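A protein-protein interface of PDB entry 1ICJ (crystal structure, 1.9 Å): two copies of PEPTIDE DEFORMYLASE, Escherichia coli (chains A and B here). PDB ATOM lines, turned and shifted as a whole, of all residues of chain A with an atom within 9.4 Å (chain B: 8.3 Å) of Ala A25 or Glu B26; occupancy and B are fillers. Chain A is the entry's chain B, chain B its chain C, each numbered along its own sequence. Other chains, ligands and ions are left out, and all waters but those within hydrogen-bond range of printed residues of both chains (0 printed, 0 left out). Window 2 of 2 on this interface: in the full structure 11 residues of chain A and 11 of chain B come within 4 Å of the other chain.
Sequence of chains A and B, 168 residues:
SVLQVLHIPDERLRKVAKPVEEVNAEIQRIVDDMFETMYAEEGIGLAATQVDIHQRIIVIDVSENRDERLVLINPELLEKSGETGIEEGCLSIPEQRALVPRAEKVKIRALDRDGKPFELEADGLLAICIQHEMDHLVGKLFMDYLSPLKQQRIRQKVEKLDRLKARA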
ATOM      1  N   VAL A  20      -2.713  15.425 -22.949  1.00  0.00           N
ATOM      2  CA  VAL A  20      -2.929  16.629 -22.166  1.00  0.00           C
ATOM      3  C   VAL A  20      -2.918  17.850 -23.102  1.00  0.00           C
ATOM      4  O   VAL A  20      -1.989  18.014 -23.894  1.00  0.00           O
ATOM      5  CB  VAL A  20      -1.829  16.747 -21.074  1.00  0.00           C
ATOM      6  CG1 VAL A  20      -1.860  18.108 -20.402  1.00  0.00           C
ATOM      7  CG2 VAL A  20      -2.013  15.642 -20.066  1.00  0.00           C
ATOM      8  N   GLU A  22      -2.999  21.150 -22.198  1.00  0.00           N
ATOM      9  CA  GLU A  22      -2.297  22.307 -21.640  1.00  0.00           C
ATOM     10  C   GLU A  22      -1.828  21.944 -20.229  1.00  0.00           C
ATOM     11  O   GLU A  22      -2.612  21.451 -19.413  1.00  0.00           O
ATOM     12  CB  GLU A  22      -3.261  23.498 -21.587  1.00  0.00           C
ATOM     13  CG  GLU A  22      -2.771  24.733 -20.848  1.00  0.00           C
ATOM     14  CD  GLU A  22      -3.916  25.693 -20.528  1.00  0.00           C
ATOM     15  OE1 GLU A  22      -4.864  25.785 -21.350  1.00  0.00           O
ATOM     16  OE2 GLU A  22      -3.910  26.302 -19.427  1.00  0.00           O
ATOM     17  N   VAL A  23      -0.531  22.078 -19.983  1.00  0.00           N
ATOM     18  CA  VAL A  23       0.007  21.806 -18.655  1.00  0.00           C
ATOM     19  C   VAL A  23      -0.252  23.000 -17.745  1.00  0.00           C
ATOM     20  O   VAL A  23       0.520  23.953 -17.722  1.00  0.00           O
ATOM     21  CB  VAL A  23       1.525  21.509 -18.696  1.00  0.00           C
ATOM     22  CG1 VAL A  23       2.039  21.235 -17.297  1.00  0.00           C
ATOM     23  CG2 VAL A  23       1.801  20.315 -19.602  1.00  0.00           C
ATOM     24  N   ASN A  24      -1.380  22.969 -17.049  1.00  0.00           N
ATOM     25  CA  ASN A  24      -1.745  24.059 -16.163  1.00  0.00           C
ATOM     26  C   ASN A  24      -1.755  23.593 -14.705  1.00  0.00           C
ATOM     27  O   ASN A  24      -1.346  22.473 -14.414  1.00  0.00           O
ATOM     28  CB  ASN A  24      -3.109  24.596 -16.574  1.00  0.00           C
ATOM     29  CG  ASN A  24      -4.133  23.520 -16.684  1.00  0.00           C
ATOM     30  OD1 ASN A  24      -4.106  22.547 -15.941  1.00  0.00           O
ATOM     31  ND2 ASN A  24      -5.041  23.669 -17.626  1.00  0.00           N
ATOM     32  N   ALA A  25      -2.286  24.421 -13.805  1.00  0.00           N
ATOM     33  CA  ALA A  25      -2.250  24.127 -12.373  1.00  0.00           C
ATOM     34  C   ALA A  25      -3.056  22.880 -12.022  1.00  0.00           C
ATOM     35  O   ALA A  25      -2.696  22.156 -11.101  1.00  0.00           O
ATOM     36  CB  ALA A  25      -2.761  25.316 -11.575  1.00  0.00           C
ATOM     37  N   GLU A  26      -4.111  22.605 -12.778  1.00  0.00           N
ATOM     38  CA  GLU A  26      -4.892  21.397 -12.549  1.00  0.00           C
ATOM     39  C   GLU A  26      -4.052  20.147 -12.806  1.00  0.00           C
ATOM     40  O   GLU A  26      -4.103  19.179 -12.036  1.00  0.00           O
ATOM     41  CB  GLU A  26      -6.112  21.371 -13.456  1.00  0.00           C
ATOM     42  CG  GLU A  26      -7.005  20.160 -13.254  1.00  0.00           C
ATOM     43  CD  GLU A  26      -7.999  19.978 -14.373  1.00  0.00           C
ATOM     44  OE1 GLU A  26      -8.124  20.873 -15.223  1.00  0.00           O
ATOM     45  OE2 GLU A  26      -8.677  18.938 -14.408  1.00  0.00           O
ATOM     46  N   ILE A  27      -3.334  20.157 -13.930  1.00  0.00           N
ATOM     47  CA  ILE A  27      -2.477  19.041 -14.317  1.00  0.00           C
ATOM     48  C   ILE A  27      -1.340  18.877 -13.310  1.00  0.00           C
ATOM     49  O   ILE A  27      -0.981  17.758 -12.937  1.00  0.00           O
ATOM     50  CB  ILE A  27      -1.877  19.256 -15.732  1.00  0.00           C
ATOM     51  CG1 ILE A  27      -2.995  19.251 -16.783  1.00  0.00           C
ATOM     52  CG2 ILE A  27      -0.818  18.192 -16.035  1.00  0.00           C
ATOM     53  CD1 ILE A  27      -3.894  18.031 -16.781  1.00  0.00           C
ATOM     54  N   GLN A  28      -0.852  19.993 -12.783  1.00  0.00           N
ATOM     55  CA  GLN A  28       0.244  19.943 -11.837  1.00  0.00           C
ATOM     56  C   GLN A  28      -0.184  19.385 -10.486  1.00  0.00           C
ATOM     57  O   GLN A  28       0.591  18.676  -9.851  1.00  0.00           O
ATOM     58  CB  GLN A  28       0.867  21.322 -11.692  1.00  0.00           C
ATOM     59  CG  GLN A  28       1.592  21.760 -12.966  1.00  0.00           C
ATOM     60  CD  GLN A  28       2.272  23.105 -12.820  1.00  0.00           C
ATOM     61  OE1 GLN A  28       1.915  23.895 -11.948  1.00  0.00           O
ATOM     62  NE2 GLN A  28       3.266  23.366 -13.665  1.00  0.00           N
ATOM     63  N   ARG A  29      -1.471  19.545 -10.151  1.00  0.00           N
ATOM     64  CA  ARG A  29      -2.038  18.961  -8.928  1.00  0.00           C
ATOM     65  C   ARG A  29      -2.146  17.448  -9.086  1.00  0.00           C
ATOM     66  O   ARG A  29      -1.800  16.688  -8.190  1.00  0.00           O
ATOM     67  CB  ARG A  29      -3.426  19.533  -8.622  1.00  0.00           C
ATOM     68  CG  ARG A  29      -4.027  18.901  -7.387  1.00  0.00           C
ATOM     69  CD  ARG A  29      -5.331  19.558  -6.929  1.00  0.00           C
ATOM     70  NE  ARG A  29      -5.149  20.920  -6.425  1.00  0.00           N
ATOM     71  CZ  ARG A  29      -4.904  21.251  -5.158  1.00  0.00           C
ATOM     72  NH1 ARG A  29      -4.686  20.327  -4.229  1.00  0.00           N
ATOM     73  NH2 ARG A  29      -4.807  22.525  -4.842  1.00  0.00           N
ATOM     74  N   ILE A  30      -2.597  17.024 -10.256  1.00  0.00           N
ATOM     75  CA  ILE A  30      -2.677  15.611 -10.594  1.00  0.00           C
ATOM     76  C   ILE A  30      -1.299  14.968 -10.493  1.00  0.00           C
ATOM     77  O   ILE A  30      -1.146  13.932  -9.854  1.00  0.00           O
ATOM     78  CB  ILE A  30      -3.256  15.399 -12.027  1.00  0.00           C
ATOM     79  CG1 ILE A  30      -4.751  15.763 -12.067  1.00  0.00           C
ATOM     80  CG2 ILE A  30      -3.051  13.961 -12.468  1.00  0.00           C
ATOM     81  CD1 ILE A  30      -5.342  15.857 -13.449  1.00  0.00           C
ATOM     82  N   VAL A  31      -0.289  15.640 -11.040  1.00  0.00           N
ATOM     83  CA  VAL A  31       1.082  15.126 -11.000  1.00  0.00           C
ATOM     84  C   VAL A  31       1.535  14.975  -9.560  1.00  0.00           C
ATOM     85  O   VAL A  31       2.067  13.933  -9.178  1.00  0.00           O
ATOM     86  CB  VAL A  31       2.080  16.062 -11.771  1.00  0.00           C
ATOM     87  CG1 VAL A  31       3.521  15.729 -11.411  1.00  0.00           C
ATOM     88  CG2 VAL A  31       1.875  15.941 -13.274  1.00  0.00           C
ATOM     89  N   ASP A  32       1.243  15.975  -8.732  1.00  0.00           N
ATOM     90  CA  ASP A  32       1.691  15.941  -7.345  1.00  0.00           C
ATOM     91  C   ASP A  32       0.959  14.880  -6.533  1.00  0.00           C
ATOM     92  O   ASP A  32       1.590  14.141  -5.795  1.00  0.00           O
ATOM     93  CB  ASP A  32       1.526  17.309  -6.690  1.00  0.00           C
ATOM     94  CG  ASP A  32       2.521  18.344  -7.215  1.00  0.00           C
ATOM     95  OD1 ASP A  32       3.544  17.969  -7.847  1.00  0.00           O
ATOM     96  OD2 ASP A  32       2.265  19.541  -6.989  1.00  0.00           O
ATOM     97  N   ASP A  33      -0.332  14.701  -6.790  1.00  0.00           N
ATOM     98  CA  ASP A  33      -1.101  13.646  -6.134  1.00  0.00           C
ATOM     99  C   ASP A  33      -0.615  12.262  -6.560  1.00  0.00           C
ATOM    100  O   ASP A  33      -0.638  11.328  -5.758  1.00  0.00           O
ATOM    101  CB  ASP A  33      -2.585  13.757  -6.474  1.00  0.00           C
ATOM    102  CG  ASP A  33      -3.269  14.954  -5.811  1.00  0.00           C
ATOM    103  OD1 ASP A  33      -2.720  15.560  -4.872  1.00  0.00           O
ATOM    104  OD2 ASP A  33      -4.388  15.278  -6.236  1.00  0.00           O
ATOM    105  N   ARG A 113       6.901  18.720 -15.885  1.00  0.00           N
ATOM    106  CA  ARG A 113       5.867  19.283 -15.018  1.00  0.00           C
ATOM    107  C   ARG A 113       5.580  20.756 -15.316  1.00  0.00           C
ATOM    108  O   ARG A 113       4.513  21.265 -14.985  1.00  0.00           O
ATOM    109  CB  ARG A 113       6.257  19.123 -13.549  1.00  0.00           C
ATOM    110  CG  ARG A 113       5.111  19.367 -12.555  1.00  0.00           C
ATOM    111  CD  ARG A 113       5.628  19.351 -11.117  1.00  0.00           C
ATOM    112  NE  ARG A 113       4.609  19.701 -10.135  1.00  0.00           N
ATOM    113  CZ  ARG A 113       4.297  20.950  -9.800  1.00  0.00           C
ATOM    114  NH1 ARG A 113       4.845  21.971 -10.451  1.00  0.00           N
ATOM    115  NH2 ARG A 113       3.391  21.187  -8.856  1.00  0.00           N
ATOM    116  N   ASP A 114       6.514  21.420 -15.990  1.00  0.00           N
ATOM    117  CA  ASP A 114       6.309  22.793 -16.427  1.00  0.00           C
ATOM    118  C   ASP A 114       5.744  22.890 -17.835  1.00  0.00           C
ATOM    119  O   ASP A 114       5.445  23.980 -18.314  1.00  0.00           O
ATOM    120  CB  ASP A 114       7.620  23.565 -16.364  1.00  0.00           C
ATOM    121  CG  ASP A 114       8.051  23.863 -14.945  1.00  0.00           C
ATOM    122  OD1 ASP A 114       7.195  24.190 -14.101  1.00  0.00           O
ATOM    123  OD2 ASP A 114       9.261  23.787 -14.677  1.00  0.00           O
ATOM    124  N   VAL B  20     -11.353  29.896  -1.640  1.00  0.00           N
ATOM    125  CA  VAL B  20     -11.104  29.626  -3.040  1.00  0.00           C
ATOM    126  C   VAL B  20     -11.043  30.961  -3.777  1.00  0.00           C
ATOM    127  O   VAL B  20     -11.946  31.772  -3.650  1.00  0.00           O
ATOM    128  CB  VAL B  20     -12.221  28.724  -3.616  1.00  0.00           C
ATOM    129  CG1 VAL B  20     -12.108  28.615  -5.121  1.00  0.00           C
ATOM    130  CG2 VAL B  20     -12.136  27.348  -2.996  1.00  0.00           C
ATOM    131  N   GLU B  22     -10.803  31.423  -7.180  1.00  0.00           N
ATOM    132  CA  GLU B  22     -11.457  31.391  -8.486  1.00  0.00           C
ATOM    133  C   GLU B  22     -11.963  29.977  -8.729  1.00  0.00           C
ATOM    134  O   GLU B  22     -11.221  29.009  -8.537  1.00  0.00           O
ATOM    135  CB  GLU B  22     -10.437  31.780  -9.560  1.00  0.00           C
ATOM    136  CG  GLU B  22     -10.883  31.595 -11.003  1.00  0.00           C
ATOM    137  CD  GLU B  22      -9.701  31.624 -11.979  1.00  0.00           C
ATOM    138  OE1 GLU B  22      -8.719  32.368 -11.718  1.00  0.00           O
ATOM    139  OE2 GLU B  22      -9.732  30.866 -12.982  1.00  0.00           O
ATOM    140  N   VAL B  23     -13.256  29.851  -9.012  1.00  0.00           N
ATOM    141  CA  VAL B  23     -13.843  28.540  -9.277  1.00  0.00           C
ATOM    142  C   VAL B  23     -13.537  28.156 -10.718  1.00  0.00           C
ATOM    143  O   VAL B  23     -14.241  28.544 -11.636  1.00  0.00           O
ATOM    144  CB  VAL B  23     -15.382  28.528  -9.045  1.00  0.00           C
ATOM    145  CG1 VAL B  23     -15.950  27.142  -9.349  1.00  0.00           C
ATOM    146  CG2 VAL B  23     -15.694  28.905  -7.618  1.00  0.00           C
ATOM    147  N   ASN B  24     -12.438  27.449 -10.917  1.00  0.00           N
ATOM    148  CA  ASN B  24     -12.043  27.044 -12.252  1.00  0.00           C
ATOM    149  C   ASN B  24     -12.095  25.524 -12.384  1.00  0.00           C
ATOM    150  O   ASN B  24     -12.562  24.845 -11.481  1.00  0.00           O
ATOM    151  CB  ASN B  24     -10.641  27.575 -12.544  1.00  0.00           C
ATOM    152  CG  ASN B  24      -9.656  27.213 -11.477  1.00  0.00           C
ATOM    153  OD1 ASN B  24      -9.743  26.140 -10.886  1.00  0.00           O
ATOM    154  ND2 ASN B  24      -8.737  28.118 -11.190  1.00  0.00           N
ATOM    155  N   ALA B  25     -11.560  24.995 -13.481  1.00  0.00           N
ATOM    156  CA  ALA B  25     -11.627  23.560 -13.761  1.00  0.00           C
ATOM    157  C   ALA B  25     -10.882  22.716 -12.728  1.00  0.00           C
ATOM    158  O   ALA B  25     -11.270  21.586 -12.453  1.00  0.00           O
ATOM    159  CB  ALA B  25     -11.093  23.263 -15.159  1.00  0.00           C
ATOM    160  N   GLU B  26      -9.835  23.279 -12.131  1.00  0.00           N
ATOM    161  CA  GLU B  26      -9.104  22.575 -11.085  1.00  0.00           C
ATOM    162  C   GLU B  26      -9.999  22.370  -9.857  1.00  0.00           C
ATOM    163  O   GLU B  26     -10.012  21.299  -9.252  1.00  0.00           O
ATOM    164  CB  GLU B  26      -7.870  23.359 -10.673  1.00  0.00           C
ATOM    165  CG  GLU B  26      -7.055  22.673  -9.606  1.00  0.00           C
ATOM    166  CD  GLU B  26      -6.053  23.592  -8.951  1.00  0.00           C
ATOM    167  OE1 GLU B  26      -5.863  24.724  -9.429  1.00  0.00           O
ATOM    168  OE2 GLU B  26      -5.446  23.187  -7.951  1.00  0.00           O
ATOM    169  N   ILE B  27     -10.712  23.424  -9.477  1.00  0.00           N
ATOM    170  CA  ILE B  27     -11.609  23.374  -8.332  1.00  0.00           C
ATOM    171  C   ILE B  27     -12.759  22.431  -8.624  1.00  0.00           C
ATOM    172  O   ILE B  27     -13.169  21.668  -7.764  1.00  0.00           O
ATOM    173  CB  ILE B  27     -12.166  24.787  -7.994  1.00  0.00           C
ATOM    174  CG1 ILE B  27     -11.035  25.706  -7.521  1.00  0.00           C
ATOM    175  CG2 ILE B  27     -13.253  24.690  -6.944  1.00  0.00           C
ATOM    176  CD1 ILE B  27     -10.209  25.157  -6.361  1.00  0.00           C
ATOM    177  N   GLN B  28     -13.195  22.391  -9.875  1.00  0.00           N
ATOM    178  CA  GLN B  28     -14.329  21.552 -10.233  1.00  0.00           C
ATOM    179  C   GLN B  28     -13.956  20.085 -10.260  1.00  0.00           C
ATOM    180  O   GLN B  28     -14.760  19.228  -9.918  1.00  0.00           O
ATOM    181  CB  GLN B  28     -14.901  21.992 -11.575  1.00  0.00           C
ATOM    182  CG  GLN B  28     -15.576  23.353 -11.501  1.00  0.00           C
ATOM    183  CD  GLN B  28     -16.199  23.755 -12.800  1.00  0.00           C
ATOM    184  OE1 GLN B  28     -15.842  23.231 -13.848  1.00  0.00           O
ATOM    185  NE2 GLN B  28     -17.124  24.696 -12.754  1.00  0.00           N
ATOM    186  N   ARG B  29     -12.677  19.828 -10.484  1.00  0.00           N
ATOM    187  CA  ARG B  29     -12.146  18.481 -10.419  1.00  0.00           C
ATOM    188  C   ARG B  29     -12.097  17.992  -8.969  1.00  0.00           C
ATOM    189  O   ARG B  29     -12.567  16.894  -8.656  1.00  0.00           O
ATOM    190  CB  ARG B  29     -10.759  18.479 -11.046  1.00  0.00           C
ATOM    191  CG  ARG B  29     -10.044  17.184 -10.962  1.00  0.00           C
ATOM    192  CD  ARG B  29      -8.939  17.156 -11.984  1.00  0.00           C
ATOM    193  NE  ARG B  29      -8.839  15.824 -12.533  1.00  0.00           N
ATOM    194  CZ  ARG B  29      -9.318  15.445 -13.704  1.00  0.00           C
ATOM    195  NH1 ARG B  29      -9.341  16.282 -14.732  1.00  0.00           N
ATOM    196  NH2 ARG B  29      -9.527  14.160 -13.896  1.00  0.00           N
ATOM    197  N   ILE B  30     -11.631  18.860  -8.076  1.00  0.00           N
ATOM    198  CA  ILE B  30     -11.635  18.597  -6.649  1.00  0.00           C
ATOM    199  C   ILE B  30     -13.056  18.296  -6.150  1.00  0.00           C
ATOM    200  O   ILE B  30     -13.272  17.316  -5.450  1.00  0.00           O
ATOM    201  CB  ILE B  30     -11.054  19.809  -5.867  1.00  0.00           C
ATOM    202  CG1 ILE B  30      -9.543  19.932  -6.136  1.00  0.00           C
ATOM    203  CG2 ILE B  30     -11.309  19.646  -4.366  1.00  0.00           C
ATOM    204  CD1 ILE B  30      -8.917  21.226  -5.654  1.00  0.00           C
ATOM    205  N   VAL B  31     -14.019  19.115  -6.562  1.00  0.00           N
ATOM    206  CA  VAL B  31     -15.416  18.938  -6.154  1.00  0.00           C
ATOM    207  C   VAL B  31     -15.915  17.562  -6.604  1.00  0.00           C
ATOM    208  O   VAL B  31     -16.516  16.825  -5.815  1.00  0.00           O
ATOM    209  CB  VAL B  31     -16.338  20.061  -6.762  1.00  0.00           C
ATOM    210  CG1 VAL B  31     -17.809  19.672  -6.657  1.00  0.00           C
ATOM    211  CG2 VAL B  31     -16.107  21.391  -6.050  1.00  0.00           C
ATOM    212  N   ASP B  32     -15.589  17.185  -7.842  1.00  0.00           N
ATOM    213  CA  ASP B  32     -16.050  15.907  -8.385  1.00  0.00           C
ATOM    214  C   ASP B  32     -15.398  14.711  -7.692  1.00  0.00           C
ATOM    215  O   ASP B  32     -16.088  13.756  -7.344  1.00  0.00           O
ATOM    216  CB  ASP B  32     -15.814  15.845  -9.896  1.00  0.00           C
ATOM    217  CG  ASP B  32     -16.760  16.751 -10.676  1.00  0.00           C
ATOM    218  OD1 ASP B  32     -17.773  17.239 -10.121  1.00  0.00           O
ATOM    219  OD2 ASP B  32     -16.486  16.978 -11.868  1.00  0.00           O
ATOM    220  N   ASP B  33     -14.122  14.843  -7.345  1.00  0.00           N
ATOM    221  CA  ASP B  33     -13.413  13.796  -6.623  1.00  0.00           C
ATOM    222  C   ASP B  33     -13.950  13.674  -5.212  1.00  0.00           C
ATOM    223  O   ASP B  33     -13.962  12.586  -4.651  1.00  0.00           O
ATOM    224  CB  ASP B  33     -11.920  14.101  -6.539  1.00  0.00           C
ATOM    225  CG  ASP B  33     -11.189  13.921  -7.879  1.00  0.00           C
ATOM    226  OD1 ASP B  33     -11.738  13.312  -8.827  1.00  0.00           O
ATOM    227  OD2 ASP B  33     -10.026  14.362  -7.950  1.00  0.00           O
ATOM    228  N   ILE B  53      -6.905  18.870   1.332  1.00  0.00           N
ATOM    229  CA  ILE B  53      -6.995  20.027   0.441  1.00  0.00           C
ATOM    230  C   ILE B  53      -7.519  21.214   1.261  1.00  0.00           C
ATOM    231  O   ILE B  53      -8.629  21.176   1.783  1.00  0.00           O
ATOM    232  CB  ILE B  53      -7.948  19.740  -0.731  1.00  0.00           C
ATOM    233  CG1 ILE B  53      -7.408  18.572  -1.567  1.00  0.00           C
ATOM    234  CG2 ILE B  53      -8.081  20.962  -1.629  1.00  0.00           C
ATOM    235  CD1 ILE B  53      -8.404  18.051  -2.591  1.00  0.00           C
ATOM    236  N   GLN B  55      -8.678  24.192   1.264  1.00  0.00           N
ATOM    237  CA  GLN B  55      -9.478  25.252   0.682  1.00  0.00           C
ATOM    238  C   GLN B  55     -10.951  25.106   1.126  1.00  0.00           C
ATOM    239  O   GLN B  55     -11.399  24.001   1.473  1.00  0.00           O
ATOM    240  CB  GLN B  55      -9.375  25.170  -0.836  1.00  0.00           C
ATOM    241  CG  GLN B  55      -7.967  25.387  -1.308  1.00  0.00           C
ATOM    242  CD  GLN B  55      -7.907  25.648  -2.767  1.00  0.00           C
ATOM    243  OE1 GLN B  55      -8.545  26.565  -3.274  1.00  0.00           O
ATOM    244  NE2 GLN B  55      -7.174  24.819  -3.478  1.00  0.00           N
ATOM    245  N   ILE B  57     -14.104  24.313   0.641  1.00  0.00           N
ATOM    246  CA  ILE B  57     -14.976  23.544  -0.250  1.00  0.00           C
ATOM    247  C   ILE B  57     -15.639  22.431   0.559  1.00  0.00           C
ATOM    248  O   ILE B  57     -14.959  21.669   1.251  1.00  0.00           O
ATOM    249  CB  ILE B  57     -14.170  22.869  -1.377  1.00  0.00           C
ATOM    250  CG1 ILE B  57     -13.323  23.900  -2.136  1.00  0.00           C
ATOM    251  CG2 ILE B  57     -15.107  22.145  -2.320  1.00  0.00           C
ATOM    252  CD1 ILE B  57     -12.371  23.277  -3.145  1.00  0.00           C
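Hydrophobic or aromatic side chains of chain B within 4 Å of the printed part of chain A: Ala B25 and Ile B30. Of the 15 printed residues of chain A, 4 touch a printed residue of chain B. Printed residues of chain A that touch a printed residue of chain B: Ala A25, Glu A26, Arg A29 and Ile A30. Among the printed residues, 8 pairs touch across the chains.
The backbone NH of Glu A26 is in hydrogen-bond range of the side-chain amide oxygen of Asn A24 (3.2 Å). The side-chain amide oxygen (OD1) of Asn B24 lies within hydrogen-bond range of the backbone NH (N) of Glu B26.
Ala A25 touches Glu B26, and with the chains exchanged Glu A26 touches Ala B25. Glu A26 touches its own counterpart, Glu B26. Glu A26 touches Arg B29, and with the chains exchanged Arg A29 touches Glu B26. Arg A29 touches Ile B30, and with the chains exchanged Ile A30 touches Arg B29. 13 positions are printed for both chains. Of the 8 pairs that touch across the chains among the printed residues, 7 have their exchanged pair printed and touching as well.
The side-chain carboxylate (OE2) of Glu A26 lies within salt-bridge range of the guanidinium group (NH1) of Arg B29 (2.8 Å). NE of Arg A29 lies within salt-bridge range of OE2 of Glu B26, 2.7 Å away.
Ala A25 touches just one residue of chain B: Glu B26 (3.8 Å). Printed residues of chain B within 4 Å of Arg A29: Glu B26, Ile B30 and Gln B55. Printed residues of chain B within 4 Å of Ile A30: Arg B29. No residue of chain A comes within 4 Å of Asn B24. Glu B26 touches just these residues of chain A: Ala A25 (3.8 Å), Glu A26 (3.8 Å) and Arg A29 (2.7 Å). Ile B27 touches none of the printed residues of chain A. Of the printed residues of chain A, Arg B29 touches Glu A26 (2.8 Å) and Ile A30 (3.6 Å). Of the printed residues of chain A, Ile B30 touches Arg A29 (3.9 Å). Printed residues of chain A within 4 Å of Gln B55: Arg A29 (3.6 Å). The nearest residue of chain B that does not touch Ala A25 is Asn B24 (6.6 Å). The nearest residue of chain A that does not touch Glu B26 is Ile A27 (6.2 Å).
Among the printed residues, pairs that only touch across the chains: Arg A29 with Gln B55, Ile A30 with Arg B29, Glu A26 with Ala B25, Ala A25 with Glu B26, Glu A26 with Glu B26 and Arg A29 with Ile B30.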
